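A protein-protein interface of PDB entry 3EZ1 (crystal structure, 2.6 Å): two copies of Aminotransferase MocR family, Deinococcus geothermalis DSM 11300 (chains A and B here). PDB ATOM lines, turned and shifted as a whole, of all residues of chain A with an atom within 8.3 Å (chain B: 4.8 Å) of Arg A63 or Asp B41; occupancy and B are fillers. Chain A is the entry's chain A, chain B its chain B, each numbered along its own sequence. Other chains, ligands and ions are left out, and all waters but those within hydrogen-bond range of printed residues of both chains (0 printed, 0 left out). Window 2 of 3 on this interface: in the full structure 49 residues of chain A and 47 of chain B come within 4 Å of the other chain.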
ATOM      1  N   GLY A  51      24.427  23.668   7.293  1.00  0.00           N
ATOM      2  CA  GLY A  51      23.344  23.578   8.293  1.00  0.00           C
ATOM      3  C   GLY A  51      22.443  24.804   8.236  1.00  0.00           C
ATOM      4  O   GLY A  51      22.471  25.553   7.256  1.00  0.00           O
ATOM      5  N   ALA A  52      21.652  25.012   9.289  1.00  0.00           N
ATOM      6  CA  ALA A  52      20.741  26.171   9.376  1.00  0.00           C
ATOM      7  C   ALA A  52      21.473  27.526   9.399  1.00  0.00           C
ATOM      8  O   ALA A  52      20.910  28.535   8.954  1.00  0.00           O
ATOM      9  CB  ALA A  52      19.815  26.044  10.587  1.00  0.00           C
ATOM     10  N   GLU A  53      22.708  27.534   9.917  1.00  0.00           N
ATOM     11  CA  GLU A  53      23.562  28.736   9.969  1.00  0.00           C
ATOM     12  C   GLU A  53      24.286  29.065   8.646  1.00  0.00           C
ATOM     13  O   GLU A  53      24.688  30.214   8.449  1.00  0.00           O
ATOM     14  CB  GLU A  53      24.603  28.599  11.088  1.00  0.00           C
ATOM     15  N   ASP A  54      24.441  28.078   7.755  1.00  0.00           N
ATOM     16  CA  ASP A  54      25.149  28.243   6.462  1.00  0.00           C
ATOM     17  C   ASP A  54      24.189  28.284   5.254  1.00  0.00           C
ATOM     18  O   ASP A  54      24.574  27.926   4.134  1.00  0.00           O
ATOM     19  CB  ASP A  54      26.159  27.092   6.279  1.00  0.00           C
ATOM     20  CG  ASP A  54      27.001  26.835   7.522  1.00  0.00           C
ATOM     21  OD1 ASP A  54      27.436  27.801   8.183  1.00  0.00           O
ATOM     22  OD2 ASP A  54      27.228  25.651   7.835  1.00  0.00           O
ATOM     23  N   VAL A  55      22.963  28.752   5.481  1.00  0.00           N
ATOM     24  CA  VAL A  55      21.916  28.817   4.448  1.00  0.00           C
ATOM     25  C   VAL A  55      22.172  29.861   3.336  1.00  0.00           C
ATOM     26  O   VAL A  55      21.780  29.631   2.183  1.00  0.00           O
ATOM     27  CB  VAL A  55      20.512  29.027   5.110  1.00  0.00           C
ATOM     28  CG1 VAL A  55      19.477  29.492   4.118  1.00  0.00           C
ATOM     29  CG2 VAL A  55      20.063  27.749   5.805  1.00  0.00           C
ATOM     30  N   ARG A  56      22.816  30.982   3.684  1.00  0.00           N
ATOM     31  CA  ARG A  56      23.121  32.066   2.730  1.00  0.00           C
ATOM     32  C   ARG A  56      24.570  31.980   2.228  1.00  0.00           C
ATOM     33  O   ARG A  56      25.462  31.557   2.971  1.00  0.00           O
ATOM     34  CB  ARG A  56      22.873  33.443   3.366  1.00  0.00           C
ATOM     35  CG  ARG A  56      21.540  33.551   4.095  1.00  0.00           C
ATOM     36  CD  ARG A  56      21.144  34.978   4.453  1.00  0.00           C
ATOM     37  NE  ARG A  56      20.398  35.652   3.376  1.00  0.00           N
ATOM     38  CZ  ARG A  56      20.879  36.507   2.460  1.00  0.00           C
ATOM     39  NH1 ARG A  56      22.168  36.866   2.412  1.00  0.00           N
ATOM     40  NH2 ARG A  56      20.038  37.026   1.562  1.00  0.00           N
ATOM     41  N   MET A  57      24.788  32.353   0.963  1.00  0.00           N
ATOM     42  CA  MET A  57      26.137  32.389   0.352  1.00  0.00           C
ATOM     43  C   MET A  57      26.103  33.254  -0.922  1.00  0.00           C
ATOM     44  O   MET A  57      25.171  33.124  -1.719  1.00  0.00           O
ATOM     45  CB  MET A  57      26.648  30.975   0.021  1.00  0.00           C
ATOM     46  CG  MET A  57      28.172  30.891  -0.080  1.00  0.00           C
ATOM     47  SD  MET A  57      28.888  29.165  -0.686  1.00  0.00           S
ATOM     48  CE  MET A  57      28.392  29.273  -2.465  1.00  0.00           C
ATOM     49  N   LEU A  60      22.990  35.485  -1.576  1.00  0.00           N
ATOM     50  CA  LEU A  60      21.822  34.726  -2.032  1.00  0.00           C
ATOM     51  C   LEU A  60      21.422  33.697  -0.986  1.00  0.00           C
ATOM     52  O   LEU A  60      22.283  33.146  -0.295  1.00  0.00           O
ATOM     53  CB  LEU A  60      22.158  33.959  -3.320  1.00  0.00           C
ATOM     54  CG  LEU A  60      22.509  34.716  -4.601  1.00  0.00           C
ATOM     55  CD1 LEU A  60      23.116  33.766  -5.616  1.00  0.00           C
ATOM     56  CD2 LEU A  60      21.282  35.421  -5.184  1.00  0.00           C
ATOM     57  N   ASP A  61      20.120  33.433  -0.894  1.00  0.00           N
ATOM     58  CA  ASP A  61      19.590  32.386  -0.027  1.00  0.00           C
ATOM     59  C   ASP A  61      19.627  31.131  -0.911  1.00  0.00           C
ATOM     60  O   ASP A  61      18.972  31.093  -1.959  1.00  0.00           O
ATOM     61  CB  ASP A  61      18.164  32.728   0.427  1.00  0.00           C
ATOM     62  CG  ASP A  61      17.620  31.763   1.473  1.00  0.00           C
ATOM     63  OD1 ASP A  61      18.021  30.580   1.497  1.00  0.00           O
ATOM     64  OD2 ASP A  61      16.761  32.199   2.268  1.00  0.00           O
ATOM     65  N   LEU A  62      20.389  30.118  -0.489  1.00  0.00           N
ATOM     66  CA  LEU A  62      20.558  28.863  -1.263  1.00  0.00           C
ATOM     67  C   LEU A  62      19.270  28.033  -1.437  1.00  0.00           C
ATOM     68  O   LEU A  62      19.150  27.282  -2.410  1.00  0.00           O
ATOM     69  CB  LEU A  62      21.654  27.984  -0.639  1.00  0.00           C
ATOM     70  CG  LEU A  62      23.067  28.580  -0.562  1.00  0.00           C
ATOM     71  CD1 LEU A  62      23.947  27.755   0.375  1.00  0.00           C
ATOM     72  CD2 LEU A  62      23.690  28.711  -1.946  1.00  0.00           C
ATOM     73  N   ARG A  63      18.320  28.187  -0.509  1.00  0.00           N
ATOM     74  CA  ARG A  63      17.034  27.467  -0.542  1.00  0.00           C
ATOM     75  C   ARG A  63      15.974  28.100  -1.463  1.00  0.00           C
ATOM     76  O   ARG A  63      14.919  27.493  -1.658  1.00  0.00           O
ATOM     77  CB  ARG A  63      16.436  27.378   0.868  1.00  0.00           C
ATOM     78  CG  ARG A  63      17.358  26.776   1.949  1.00  0.00           C
ATOM     79  CD  ARG A  63      16.800  26.976   3.356  1.00  0.00           C
ATOM     80  NE  ARG A  63      16.700  28.394   3.728  1.00  0.00           N
ATOM     81  CZ  ARG A  63      16.189  28.887   4.857  1.00  0.00           C
ATOM     82  NH1 ARG A  63      15.664  28.090   5.784  1.00  0.00           N
ATOM     83  NH2 ARG A  63      16.180  30.210   5.053  1.00  0.00           N
ATOM     84  N   ASN A  64      16.246  29.296  -2.007  1.00  0.00           N
ATOM     85  CA  ASN A  64      15.313  30.040  -2.871  1.00  0.00           C
ATOM     86  C   ASN A  64      15.800  30.066  -4.335  1.00  0.00           C
ATOM     87  O   ASN A  64      16.974  29.796  -4.605  1.00  0.00           O
ATOM     88  CB  ASN A  64      15.154  31.472  -2.305  1.00  0.00           C
ATOM     89  CG  ASN A  64      13.866  32.178  -2.759  1.00  0.00           C
ATOM     90  OD1 ASN A  64      13.117  31.689  -3.607  1.00  0.00           O
ATOM     91  ND2 ASN A  64      13.614  33.341  -2.177  1.00  0.00           N
ATOM     92  N   TYR A  65      14.876  30.366  -5.256  1.00  0.00           N
ATOM     93  CA  TYR A  65      15.146  30.429  -6.713  1.00  0.00           C
ATOM     94  C   TYR A  65      16.237  31.388  -7.239  1.00  0.00           C
ATOM     95  O   TYR A  65      17.020  30.970  -8.093  1.00  0.00           O
ATOM     96  CB  TYR A  65      13.854  30.717  -7.519  1.00  0.00           C
ATOM     97  CG  TYR A  65      12.839  29.585  -7.614  1.00  0.00           C
ATOM     98  CD1 TYR A  65      13.194  28.332  -8.144  1.00  0.00           C
ATOM     99  CD2 TYR A  65      11.495  29.793  -7.272  1.00  0.00           C
ATOM    100  CE1 TYR A  65      12.248  27.295  -8.268  1.00  0.00           C
ATOM    101  CE2 TYR A  65      10.537  28.768  -7.396  1.00  0.00           C
ATOM    102  CZ  TYR A  65      10.919  27.526  -7.894  1.00  0.00           C
ATOM    103  OH  TYR A  65       9.974  26.537  -8.016  1.00  0.00           O
ATOM    104  N   PRO A  66      16.273  32.667  -6.776  1.00  0.00           N
ATOM    105  CA  PRO A  66      17.241  33.659  -7.292  1.00  0.00           C
ATOM    106  C   PRO A  66      18.722  33.241  -7.256  1.00  0.00           C
ATOM    107  O   PRO A  66      19.145  32.589  -6.300  1.00  0.00           O
ATOM    108  CB  PRO A  66      17.008  34.874  -6.384  1.00  0.00           C
ATOM    109  CG  PRO A  66      15.629  34.749  -5.949  1.00  0.00           C
ATOM    110  CD  PRO A  66      15.416  33.284  -5.745  1.00  0.00           C
ATOM    111  N   ASN A 286      21.025  23.114  -8.855  1.00  0.00           N
ATOM    112  CA  ASN A 286      20.965  22.892  -7.405  1.00  0.00           C
ATOM    113  C   ASN A 286      22.071  23.717  -6.749  1.00  0.00           C
ATOM    114  O   ASN A 286      23.253  23.388  -6.811  1.00  0.00           O
ATOM    115  CB  ASN A 286      21.049  21.410  -7.022  1.00  0.00           C
ATOM    116  CG  ASN A 286      20.627  21.149  -5.576  1.00  0.00           C
ATOM    117  OD1 ASN A 286      20.919  21.927  -4.664  1.00  0.00           O
ATOM    118  ND2 ASN A 286      19.937  20.038  -5.364  1.00  0.00           N
ATOM    119  N   LYS A 287      21.635  24.790  -6.110  1.00  0.00           N
ATOM    120  CA  LYS A 287      22.507  25.798  -5.515  1.00  0.00           C
ATOM    121  C   LYS A 287      23.037  25.331  -4.144  1.00  0.00           C
ATOM    122  O   LYS A 287      24.115  25.752  -3.724  1.00  0.00           O
ATOM    123  CB  LYS A 287      21.690  27.097  -5.428  1.00  0.00           C
ATOM    124  CG  LYS A 287      22.421  28.419  -5.542  1.00  0.00           C
ATOM    125  CD  LYS A 287      21.487  29.501  -6.124  1.00  0.00           C
ATOM    126  CE  LYS A 287      20.190  29.728  -5.322  1.00  0.00           C
ATOM    127  NZ  LYS A 287      19.067  30.019  -6.242  1.00  0.00           N
ATOM    128  N   VAL A 288      22.283  24.455  -3.469  1.00  0.00           N
ATOM    129  CA  VAL A 288      22.668  23.901  -2.162  1.00  0.00           C
ATOM    130  C   VAL A 288      23.828  22.910  -2.317  1.00  0.00           C
ATOM    131  O   VAL A 288      24.766  22.945  -1.518  1.00  0.00           O
ATOM    132  CB  VAL A 288      21.452  23.260  -1.413  1.00  0.00           C
ATOM    133  CG1 VAL A 288      21.869  22.679  -0.073  1.00  0.00           C
ATOM    134  CG2 VAL A 288      20.361  24.302  -1.192  1.00  0.00           C
ATOM    135  N   ASP B  37      10.683  33.115   3.866  1.00  0.00           N
ATOM    136  CA  ASP B  37      11.784  32.567   4.686  1.00  0.00           C
ATOM    137  C   ASP B  37      11.233  31.556   5.691  1.00  0.00           C
ATOM    138  O   ASP B  37      11.859  30.525   5.923  1.00  0.00           O
ATOM    139  CB  ASP B  37      12.578  33.660   5.421  1.00  0.00           C
ATOM    140  CG  ASP B  37      13.487  34.470   4.504  1.00  0.00           C
ATOM    141  OD1 ASP B  37      13.981  33.954   3.485  1.00  0.00           O
ATOM    142  OD2 ASP B  37      13.754  35.638   4.841  1.00  0.00           O
ATOM    143  N   ALA B  38      10.061  31.854   6.262  1.00  0.00           N
ATOM    144  CA  ALA B  38       9.366  30.949   7.193  1.00  0.00           C
ATOM    145  C   ALA B  38       9.038  29.580   6.569  1.00  0.00           C
ATOM    146  O   ALA B  38       9.044  28.570   7.281  1.00  0.00           O
ATOM    147  CB  ALA B  38       8.096  31.604   7.734  1.00  0.00           C
ATOM    148  N   ASP B  39       8.752  29.555   5.258  1.00  0.00           N
ATOM    149  CA  ASP B  39       8.490  28.302   4.524  1.00  0.00           C
ATOM    150  C   ASP B  39       9.758  27.464   4.436  1.00  0.00           C
ATOM    151  O   ASP B  39       9.720  26.263   4.717  1.00  0.00           O
ATOM    152  CB  ASP B  39       7.975  28.564   3.100  1.00  0.00           C
ATOM    153  CG  ASP B  39       6.599  29.191   3.075  1.00  0.00           C
ATOM    154  OD1 ASP B  39       5.691  28.683   3.765  1.00  0.00           O
ATOM    155  OD2 ASP B  39       6.416  30.177   2.335  1.00  0.00           O
ATOM    156  N   PHE B  40      10.866  28.104   4.050  1.00  0.00           N
ATOM    157  CA  PHE B  40      12.167  27.425   3.934  1.00  0.00           C
ATOM    158  C   PHE B  40      12.685  26.920   5.290  1.00  0.00           C
ATOM    159  O   PHE B  40      13.335  25.875   5.333  1.00  0.00           O
ATOM    160  CB  PHE B  40      13.248  28.316   3.297  1.00  0.00           C
ATOM    161  CG  PHE B  40      12.894  28.862   1.936  1.00  0.00           C
ATOM    162  CD1 PHE B  40      12.501  28.011   0.897  1.00  0.00           C
ATOM    163  CD2 PHE B  40      13.012  30.232   1.671  1.00  0.00           C
ATOM    164  CE1 PHE B  40      12.183  28.525  -0.374  1.00  0.00           C
ATOM    165  CE2 PHE B  40      12.701  30.756   0.406  1.00  0.00           C
ATOM    166  CZ  PHE B  40      12.287  29.902  -0.619  1.00  0.00           C
ATOM    167  N   ASP B  41      12.407  27.669   6.371  1.00  0.00           N
ATOM    168  CA  ASP B  41      12.792  27.287   7.756  1.00  0.00           C
ATOM    169  C   ASP B  41      12.266  25.898   8.148  1.00  0.00           C
ATOM    170  O   ASP B  41      12.970  25.146   8.821  1.00  0.00           O
ATOM    171  CB  ASP B  41      12.288  28.311   8.808  1.00  0.00           C
ATOM    172  CG  ASP B  41      12.999  29.675   8.745  1.00  0.00           C
ATOM    173  OD1 ASP B  41      14.002  29.849   8.024  1.00  0.00           O
ATOM    174  OD2 ASP B  41      12.533  30.597   9.451  1.00  0.00           O
ATOM    175  N   LEU B  42      11.041  25.573   7.714  1.00  0.00           N
ATOM    176  CA  LEU B  42      10.405  24.268   7.985  1.00  0.00           C
ATOM    177  C   LEU B  42      11.206  23.061   7.478  1.00  0.00           C
ATOM    178  O   LEU B  42      11.139  21.989   8.082  1.00  0.00           O
ATOM    179  CB  LEU B  42       8.988  24.199   7.377  1.00  0.00           C
ATOM    180  CG  LEU B  42       7.924  25.188   7.873  1.00  0.00           C
ATOM    181  CD1 LEU B  42       6.670  25.123   7.004  1.00  0.00           C
ATOM    182  CD2 LEU B  42       7.585  24.949   9.341  1.00  0.00           C
ATOM    183  N   SER B  43      11.957  23.251   6.391  1.00  0.00           N
ATOM    184  CA  SER B  43      12.746  22.182   5.756  1.00  0.00           C
ATOM    185  C   SER B  43      14.261  22.170   6.049  1.00  0.00           C
ATOM    186  O   SER B  43      14.997  21.449   5.378  1.00  0.00           O
ATOM    187  CB  SER B  43      12.472  22.194   4.243  1.00  0.00           C
ATOM    188  OG  SER B  43      11.074  22.095   4.002  1.00  0.00           O
ATOM    189  N   ASN B  44      14.717  22.921   7.060  1.00  0.00           N
ATOM    190  CA  ASN B  44      16.154  22.953   7.438  1.00  0.00           C
ATOM    191  C   ASN B  44      16.755  21.611   7.884  1.00  0.00           C
ATOM    192  O   ASN B  44      17.966  21.417   7.761  1.00  0.00           O
ATOM    193  CB  ASN B  44      16.453  24.043   8.498  1.00  0.00           C
ATOM    194  CG  ASN B  44      16.575  25.442   7.902  1.00  0.00           C
ATOM    195  OD1 ASN B  44      16.990  25.610   6.760  1.00  0.00           O
ATOM    196  ND2 ASN B  44      16.269  26.453   8.705  1.00  0.00           N
ATOM    197  N   PHE B 256      12.903  22.867  -0.708  1.00  0.00           N
ATOM    198  CA  PHE B 256      13.620  24.098  -1.105  1.00  0.00           C
ATOM    199  C   PHE B 256      13.376  24.433  -2.581  1.00  0.00           C
ATOM    200  O   PHE B 256      13.474  23.546  -3.434  1.00  0.00           O
ATOM    201  CB  PHE B 256      15.141  23.967  -0.918  1.00  0.00           C
ATOM    202  CG  PHE B 256      15.589  23.589   0.477  1.00  0.00           C
ATOM    203  CD1 PHE B 256      15.027  24.177   1.620  1.00  0.00           C
ATOM    204  CD2 PHE B 256      16.665  22.708   0.643  1.00  0.00           C
ATOM    205  CE1 PHE B 256      15.483  23.831   2.906  1.00  0.00           C
ATOM    206  CE2 PHE B 256      17.133  22.365   1.922  1.00  0.00           C
ATOM    207  CZ  PHE B 256      16.543  22.930   3.054  1.00  0.00           C
ATOM    208  N   ALA B 257      13.112  25.714  -2.875  1.00  0.00           N
ATOM    209  CA  ALA B 257      12.891  26.201  -4.247  1.00  0.00           C
ATOM    210  C   ALA B 257      14.232  26.256  -4.970  1.00  0.00           C
ATOM    211  O   ALA B 257      15.106  27.031  -4.589  1.00  0.00           O
ATOM    212  CB  ALA B 257      12.238  27.576  -4.238  1.00  0.00           C
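O of Val A55 is in hydrogen-bond range of N of Leu A62, at 3.1 Å.
NE of Arg A63 lies within salt-bridge range of OD1 of Asp A61 (3.4 Å).
The backbone carbonyl oxygen (O) of Asn A64 lies within hydrogen-bond range of the side-chain amino group (NZ) of Lys A287, at 2.7 Å.
NZ of Lys A287 is in hydrogen-bond range of O of Tyr A65 (2.9 Å).
The guanidinium group (NH1) of Arg A63 lies close to the backbone carbonyl oxygen (O) of Phe B40 (3.2 Å).
NH1 of Arg A63 is in salt-bridge range of OD1 of Asp B41 (3.3 Å).
NH1 of Arg A63 is in hydrogen-bond range of OD1 of Asn B44 (3.0 Å).
The backbone carbonyl oxygen (O) of Arg A63 sits at hydrogen-bond distance from the backbone NH (N) of Ala B257 (2.8 Å).
The backbone NH (N) of Tyr A65 lies within hydrogen-bond range of the backbone carbonyl oxygen (O) of Ala B257.
The backbone carbonyl oxygen (O) of Ala B257 sits close to the backbone carbonyl oxygen (O) of Asn A64 (3.3 Å).
No position is printed for both chains.
Of the printed residues of chain B, Arg A63 touches Phe B40 (3.2 Å), Asp B41 (3.3 Å), Asn B44 (3.0 Å), Phe B256 (3.4 Å) and Ala B257 (2.8 Å).
Asp B41 touches just one residue of chain A: Arg A63.
Of chain A, only Arg A63 (2.8 Å), Asn A64 (3.1 Å) and Tyr A65 (3.4 Å) come within 4 Å of Ala B257.
Of the printed residues of chain A, Phe B256 touches Arg A63.
Of the printed residues of chain A, Asp B37 touches Asp A61 (3.5 Å).
Of the printed residues of chain A, Phe B40 touches Arg A63 (3.2 Å) and Asn A64 (3.5 Å).
The nearest residue of chain A that does not touch Asp B41 is Val A55 (6.7 Å).
The nearest printed residue of chain A that does not touch Asn B44 is Ala A52 (4.04 Å).
Among the printed residues, pairs that only touch across the chains: Val A55 with Asn B44 (3.9 Å), Asp A61 with Asp B37 (3.5 Å), Arg A63 with Phe B256 (3.4 Å) and Asn A64 with Phe B40 (3.5 Å).
Printed residues of chain A that touch a printed residue of chain B: Val A55, Asp A61, Arg A63, Asn A64 and Tyr A65.
Hydrophobic or aromatic side chains of chain A within 4 Å of the printed part of chain B: Val A55 and Tyr A65.
Along chain A the printed residues that touch a printed residue of chain B span positions 55 to 65.
Of the 10 printed residues of chain B, 6 touch a printed residue of chain A.
Along chain B the printed residues that touch a printed residue of chain A span positions 37 to 257.
Among the printed residues, 10 pairs touch across the chains.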
